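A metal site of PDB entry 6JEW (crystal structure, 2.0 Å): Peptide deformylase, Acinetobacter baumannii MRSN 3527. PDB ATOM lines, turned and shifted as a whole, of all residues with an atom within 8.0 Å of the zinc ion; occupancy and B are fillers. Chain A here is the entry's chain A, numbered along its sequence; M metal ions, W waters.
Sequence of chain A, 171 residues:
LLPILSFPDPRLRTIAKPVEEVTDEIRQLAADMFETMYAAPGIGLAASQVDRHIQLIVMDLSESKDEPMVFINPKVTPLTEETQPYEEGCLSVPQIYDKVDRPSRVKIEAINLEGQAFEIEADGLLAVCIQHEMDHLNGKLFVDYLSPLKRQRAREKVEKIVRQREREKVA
The zinc ion is bound by a ring nitrogen (NE2) of His 136 (2.0 Å), a ring nitrogen (NE2) of His 132 (2.0 Å) and the side-chain sulfur of Cys 90 (2.3 Å). The zinc ion has three donor atoms within binding distance.
A ring nitrogen (ND1) of His 132 sits at hydrogen-bond distance from the side-chain carboxylate (OE1) of Glu 88 (2.7 Å). The side-chain amide oxygen (OE1) of Gln 49 is in hydrogen-bond range of the backbone NH (N) of Ala 46 (3.0 Å). A ring nitrogen (NE2) of His 136 lies close to the side-chain amide oxygen (OE1) of Gln 49 (3.4 Å). The side-chain sulfur of Cys 90 sits close to the side-chain amide nitrogen of Gln 49. The side-chain amide oxygen (OE1) of Gln 49 lies close to the side-chain carboxylate (OE1) of Glu 133. The side-chain amide nitrogen of Gln 49 lies within hydrogen-bond range of the side-chain hydroxyl of Ser 92, 2.7 Å away. N of Ser 92 lies close to SG of Cys 90, 3.4 Å away.
Residues that only touch the zinc ion: Gln 49. Of the 22 residues printed, 4 come within 4 Å of the zinc ion.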
ATOM      1  N   ILE A   4     -19.803  11.985  -5.043  1.00  0.00           N
ATOM      2  CA  ILE A   4     -20.116  11.601  -6.418  1.00  0.00           C
ATOM      3  C   ILE A   4     -18.988  12.043  -7.332  1.00  0.00           C
ATOM      4  O   ILE A   4     -18.630  13.208  -7.296  1.00  0.00           O
ATOM      5  CB  ILE A   4     -21.426  12.251  -6.864  1.00  0.00           C
ATOM      6  CG1 ILE A   4     -22.563  11.687  -6.031  1.00  0.00           C
ATOM      7  CG2 ILE A   4     -21.730  11.981  -8.338  1.00  0.00           C
ATOM      8  CD1 ILE A   4     -23.832  12.522  -6.149  1.00  0.00           C
ATOM      9  N   LEU A  12     -15.017   7.082 -13.936  1.00  0.00           N
ATOM     10  CA  LEU A  12     -16.426   6.949 -14.432  1.00  0.00           C
ATOM     11  C   LEU A  12     -16.519   6.085 -15.673  1.00  0.00           C
ATOM     12  O   LEU A  12     -17.623   5.787 -16.134  1.00  0.00           O
ATOM     13  CB  LEU A  12     -17.060   8.322 -14.714  1.00  0.00           C
ATOM     14  CG  LEU A  12     -17.437   9.107 -13.454  1.00  0.00           C
ATOM     15  CD1 LEU A  12     -17.446  10.589 -13.761  1.00  0.00           C
ATOM     16  CD2 LEU A  12     -18.790   8.638 -12.900  1.00  0.00           C
ATOM     17  N   GLY A  44     -31.672   8.985  -9.743  1.00  0.00           N
ATOM     18  CA  GLY A  44     -30.980   7.756 -10.106  1.00  0.00           C
ATOM     19  C   GLY A  44     -29.515   7.903  -9.783  1.00  0.00           C
ATOM     20  O   GLY A  44     -28.949   9.025  -9.814  1.00  0.00           O
ATOM     21  N   LEU A  45     -28.907   6.815  -9.342  1.00  0.00           N
ATOM     22  CA  LEU A  45     -27.471   6.804  -9.089  1.00  0.00           C
ATOM     23  C   LEU A  45     -26.946   5.369  -9.209  1.00  0.00           C
ATOM     24  O   LEU A  45     -27.528   4.427  -8.600  1.00  0.00           O
ATOM     25  CB  LEU A  45     -27.202   7.396  -7.718  1.00  0.00           C
ATOM     26  CG  LEU A  45     -25.739   7.581  -7.281  1.00  0.00           C
ATOM     27  CD1 LEU A  45     -25.147   8.770  -8.015  1.00  0.00           C
ATOM     28  CD2 LEU A  45     -25.740   7.851  -5.782  1.00  0.00           C
ATOM     29  N   ALA A  46     -25.862   5.209 -10.008  1.00  0.00           N
ATOM     30  CA  ALA A  46     -25.188   3.931 -10.246  1.00  0.00           C
ATOM     31  C   ALA A  46     -23.986   3.916  -9.319  1.00  0.00           C
ATOM     32  O   ALA A  46     -23.375   4.964  -9.063  1.00  0.00           O
ATOM     33  CB  ALA A  46     -24.726   3.784 -11.698  1.00  0.00           C
ATOM     34  N   GLN A  49     -20.705   5.759  -9.948  1.00  0.00           N
ATOM     35  CA  GLN A  49     -20.692   7.197  -9.582  1.00  0.00           C
ATOM     36  C   GLN A  49     -20.173   7.565  -8.192  1.00  0.00           C
ATOM     37  O   GLN A  49     -19.822   8.724  -7.929  1.00  0.00           O
ATOM     38  CB  GLN A  49     -22.092   7.807  -9.736  1.00  0.00           C
ATOM     39  CG  GLN A  49     -22.509   7.845 -11.175  1.00  0.00           C
ATOM     40  CD  GLN A  49     -23.866   8.438 -11.335  1.00  0.00           C
ATOM     41  OE1 GLN A  49     -24.859   7.691 -11.467  1.00  0.00           O
ATOM     42  NE2 GLN A  49     -23.933   9.776 -11.412  1.00  0.00           N
ATOM     43  N   GLU A  88     -32.237  14.750 -20.290  1.00  0.00           N
ATOM     44  CA  GLU A  88     -31.477  14.014 -19.258  1.00  0.00           C
ATOM     45  C   GLU A  88     -30.463  14.883 -18.558  1.00  0.00           C
ATOM     46  O   GLU A  88     -29.738  15.638 -19.218  1.00  0.00           O
ATOM     47  CB  GLU A  88     -30.674  12.858 -19.881  1.00  0.00           C
ATOM     48  CG  GLU A  88     -31.489  11.640 -20.230  1.00  0.00           C
ATOM     49  CD  GLU A  88     -30.658  10.490 -20.763  1.00  0.00           C
ATOM     50  OE1 GLU A  88     -29.570  10.181 -20.233  1.00  0.00           O
ATOM     51  OE2 GLU A  88     -31.122   9.810 -21.700  1.00  0.00           O
ATOM     52  N   GLY A  89     -30.387  14.728 -17.232  1.00  0.00           N
ATOM     53  CA  GLY A  89     -29.225  15.139 -16.479  1.00  0.00           C
ATOM     54  C   GLY A  89     -28.522  13.965 -15.807  1.00  0.00           C
ATOM     55  O   GLY A  89     -28.823  12.775 -16.102  1.00  0.00           O
ATOM     56  N   CYS A  90     -27.619  14.300 -14.875  1.00  0.00           N
ATOM     57  CA  CYS A  90     -26.740  13.310 -14.267  1.00  0.00           C
ATOM     58  C   CYS A  90     -25.986  13.953 -13.130  1.00  0.00           C
ATOM     59  O   CYS A  90     -25.300  14.926 -13.340  1.00  0.00           O
ATOM     60  CB  CYS A  90     -25.722  12.726 -15.297  1.00  0.00           C
ATOM     61  SG  CYS A  90     -24.632  11.443 -14.587  1.00  0.00           S
ATOM     62  N   LEU A  91     -26.039  13.353 -11.944  1.00  0.00           N
ATOM     63  CA  LEU A  91     -25.307  13.881 -10.811  1.00  0.00           C
ATOM     64  C   LEU A  91     -23.820  13.884 -11.049  1.00  0.00           C
ATOM     65  O   LEU A  91     -23.124  14.593 -10.349  1.00  0.00           O
ATOM     66  CB  LEU A  91     -25.629  13.111  -9.518  1.00  0.00           C
ATOM     67  CG  LEU A  91     -27.134  13.207  -9.161  1.00  0.00           C
ATOM     68  CD1 LEU A  91     -27.368  12.378  -7.901  1.00  0.00           C
ATOM     69  CD2 LEU A  91     -27.588  14.630  -8.957  1.00  0.00           C
ATOM     70  N   SER A  92     -23.303  13.121 -11.979  1.00  0.00           N
ATOM     71  CA  SER A  92     -21.874  13.146 -12.298  1.00  0.00           C
ATOM     72  C   SER A  92     -21.541  14.125 -13.448  1.00  0.00           C
ATOM     73  O   SER A  92     -20.348  14.222 -13.868  1.00  0.00           O
ATOM     74  CB  SER A  92     -21.378  11.729 -12.619  1.00  0.00           C
ATOM     75  OG  SER A  92     -21.449  10.890 -11.475  1.00  0.00           O
ATOM     76  N   VAL A  93     -22.568  14.793 -13.981  1.00  0.00           N
ATOM     77  CA  VAL A  93     -22.439  15.918 -14.921  1.00  0.00           C
ATOM     78  C   VAL A  93     -23.293  17.089 -14.389  1.00  0.00           C
ATOM     79  O   VAL A  93     -24.294  17.509 -14.997  1.00  0.00           O
ATOM     80  CB  VAL A  93     -22.850  15.513 -16.345  1.00  0.00           C
ATOM     81  CG1 VAL A  93     -22.327  16.519 -17.349  1.00  0.00           C
ATOM     82  CG2 VAL A  93     -22.301  14.154 -16.679  1.00  0.00           C
ATOM     83  N   ARG A 102     -33.446   7.548 -26.858  1.00  0.00           N
ATOM     84  CA  ARG A 102     -33.236   6.163 -26.428  1.00  0.00           C
ATOM     85  C   ARG A 102     -34.436   5.300 -26.799  1.00  0.00           C
ATOM     86  O   ARG A 102     -35.569   5.787 -26.779  1.00  0.00           O
ATOM     87  CB  ARG A 102     -33.095   6.119 -24.907  1.00  0.00           C
ATOM     88  CG  ARG A 102     -32.078   7.085 -24.318  1.00  0.00           C
ATOM     89  CD  ARG A 102     -31.590   6.562 -22.959  1.00  0.00           C
ATOM     90  NE  ARG A 102     -30.545   7.384 -22.304  1.00  0.00           N
ATOM     91  CZ  ARG A 102     -29.269   7.020 -22.118  1.00  0.00           C
ATOM     92  NH1 ARG A 102     -28.779   5.904 -22.607  1.00  0.00           N
ATOM     93  NH2 ARG A 102     -28.422   7.828 -21.479  1.00  0.00           N
ATOM     94  N   CYS A 129     -34.394   6.213 -17.575  1.00  0.00           N
ATOM     95  CA  CYS A 129     -33.519   6.227 -16.414  1.00  0.00           C
ATOM     96  C   CYS A 129     -32.726   4.960 -16.287  1.00  0.00           C
ATOM     97  O   CYS A 129     -31.513   5.034 -16.072  1.00  0.00           O
ATOM     98  CB  CYS A 129     -34.331   6.453 -15.133  1.00  0.00           C
ATOM     99  SG  CYS A 129     -33.261   6.836 -13.745  1.00  0.00           S
ATOM    100  N   HIS A 132     -30.028   5.033 -18.830  1.00  0.00           N
ATOM    101  CA  HIS A 132     -29.002   5.974 -18.433  1.00  0.00           C
ATOM    102  C   HIS A 132     -28.098   5.346 -17.392  1.00  0.00           C
ATOM    103  O   HIS A 132     -26.890   5.392 -17.503  1.00  0.00           O
ATOM    104  CB  HIS A 132     -29.655   7.262 -17.949  1.00  0.00           C
ATOM    105  CG  HIS A 132     -28.703   8.253 -17.345  1.00  0.00           C
ATOM    106  ND1 HIS A 132     -28.343   9.410 -17.976  1.00  0.00           N
ATOM    107  CD2 HIS A 132     -28.032   8.247 -16.151  1.00  0.00           C
ATOM    108  CE1 HIS A 132     -27.468  10.071 -17.226  1.00  0.00           C
ATOM    109  NE2 HIS A 132     -27.277   9.398 -16.109  1.00  0.00           N
ATOM    110  N   GLU A 133     -28.681   4.717 -16.363  1.00  0.00           N
ATOM    111  CA  GLU A 133     -27.863   4.114 -15.314  1.00  0.00           C
ATOM    112  C   GLU A 133     -27.048   2.849 -15.711  1.00  0.00           C
ATOM    113  O   GLU A 133     -25.880   2.676 -15.275  1.00  0.00           O
ATOM    114  CB  GLU A 133     -28.730   3.837 -14.073  1.00  0.00           C
ATOM    115  CG  GLU A 133     -29.437   5.050 -13.522  1.00  0.00           C
ATOM    116  CD  GLU A 133     -28.502   6.121 -13.085  1.00  0.00           C
ATOM    117  OE1 GLU A 133     -27.342   5.804 -12.692  1.00  0.00           O
ATOM    118  OE2 GLU A 133     -28.937   7.313 -13.150  1.00  0.00           O
ATOM    119  N   MET A 134     -27.611   2.015 -16.568  1.00  0.00           N
ATOM    120  CA  MET A 134     -26.908   0.875 -17.155  1.00  0.00           C
ATOM    121  C   MET A 134     -25.674   1.329 -17.956  1.00  0.00           C
ATOM    122  O   MET A 134     -24.626   0.684 -17.912  1.00  0.00           O
ATOM    123  CB  MET A 134     -27.813   0.108 -18.077  1.00  0.00           C
ATOM    124  CG  MET A 134     -27.228  -1.244 -18.565  1.00  0.00           C
ATOM    125  SD  MET A 134     -27.219  -2.446 -17.213  1.00  0.00           S
ATOM    126  CE  MET A 134     -28.935  -2.846 -17.217  1.00  0.00           C
ATOM    127  N   ASP A 135     -25.821   2.433 -18.657  1.00  0.00           N
ATOM    128  CA  ASP A 135     -24.654   3.104 -19.288  1.00  0.00           C
ATOM    129  C   ASP A 135     -23.541   3.354 -18.318  1.00  0.00           C
ATOM    130  O   ASP A 135     -22.397   3.097 -18.645  1.00  0.00           O
ATOM    131  CB  ASP A 135     -25.107   4.412 -19.982  1.00  0.00           C
ATOM    132  CG  ASP A 135     -25.596   4.158 -21.434  1.00  0.00           C
ATOM    133  OD1 ASP A 135     -25.466   3.011 -21.876  1.00  0.00           O
ATOM    134  OD2 ASP A 135     -26.075   5.090 -22.137  1.00  0.00           O
ATOM    135  N   HIS A 136     -23.826   3.822 -17.103  1.00  0.00           N
ATOM    136  CA  HIS A 136     -22.784   4.056 -16.092  1.00  0.00           C
ATOM    137  C   HIS A 136     -22.006   2.803 -15.739  1.00  0.00           C
ATOM    138  O   HIS A 136     -20.748   2.837 -15.522  1.00  0.00           O
ATOM    139  CB  HIS A 136     -23.364   4.632 -14.760  1.00  0.00           C
ATOM    140  CG  HIS A 136     -23.684   6.084 -14.807  1.00  0.00           C
ATOM    141  ND1 HIS A 136     -22.708   7.057 -14.939  1.00  0.00           N
ATOM    142  CD2 HIS A 136     -24.860   6.741 -14.699  1.00  0.00           C
ATOM    143  CE1 HIS A 136     -23.285   8.245 -14.944  1.00  0.00           C
ATOM    144  NE2 HIS A 136     -24.588   8.088 -14.792  1.00  0.00           N
ATOM    145  N   LYS A 140     -20.168   4.573 -19.393  1.00  0.00           N
ATOM    146  CA  LYS A 140     -20.665   5.595 -20.291  1.00  0.00           C
ATOM    147  C   LYS A 140     -21.536   6.670 -19.618  1.00  0.00           C
ATOM    148  O   LYS A 140     -22.303   6.388 -18.660  1.00  0.00           O
ATOM    149  CB  LYS A 140     -21.485   4.981 -21.397  1.00  0.00           C
ATOM    150  CG  LYS A 140     -20.714   4.072 -22.322  1.00  0.00           C
ATOM    151  CD  LYS A 140     -21.623   3.395 -23.334  1.00  0.00           C
ATOM    152  CE  LYS A 140     -22.635   4.361 -23.955  1.00  0.00           C
ATOM    153  NZ  LYS A 140     -23.217   3.813 -25.206  1.00  0.00           N
ATOM    154  N   LEU A 141     -21.433   7.880 -20.186  1.00  0.00           N
ATOM    155  CA  LEU A 141     -22.137   9.043 -19.710  1.00  0.00           C
ATOM    156  C   LEU A 141     -23.009   9.594 -20.804  1.00  0.00           C
ATOM    157  O   LEU A 141     -22.688   9.431 -21.950  1.00  0.00           O
ATOM    158  CB  LEU A 141     -21.131  10.104 -19.262  1.00  0.00           C
ATOM    159  CG  LEU A 141     -20.037   9.656 -18.272  1.00  0.00           C
ATOM    160  CD1 LEU A 141     -18.996  10.750 -18.103  1.00  0.00           C
ATOM    161  CD2 LEU A 141     -20.703   9.312 -16.950  1.00  0.00           C
ATOM    162  N   PHE A 142     -24.096  10.293 -20.441  1.00  0.00           N
ATOM    163  CA  PHE A 142     -25.085  10.757 -21.434  1.00  0.00           C
ATOM    164  C   PHE A 142     -24.559  11.871 -22.383  1.00  0.00           C
ATOM    165  O   PHE A 142     -25.128  12.114 -23.448  1.00  0.00           O
ATOM    166  CB  PHE A 142     -26.359  11.202 -20.746  1.00  0.00           C
ATOM    167  CG  PHE A 142     -26.333  12.664 -20.285  1.00  0.00           C
ATOM    168  CD1 PHE A 142     -25.749  13.024 -19.068  1.00  0.00           C
ATOM    169  CD2 PHE A 142     -26.921  13.656 -21.065  1.00  0.00           C
ATOM    170  CE1 PHE A 142     -25.746  14.359 -18.674  1.00  0.00           C
ATOM    171  CE2 PHE A 142     -26.917  14.987 -20.658  1.00  0.00           C
ATOM    172  CZ  PHE A 142     -26.333  15.332 -19.460  1.00  0.00           C
HETATM  173 ZN    ZN M   1     -25.892   9.552 -14.609  1.00  0.00          ZN
HETATM  174  O   HOH W   1     -24.441  10.145 -17.609  1.00  0.00           O
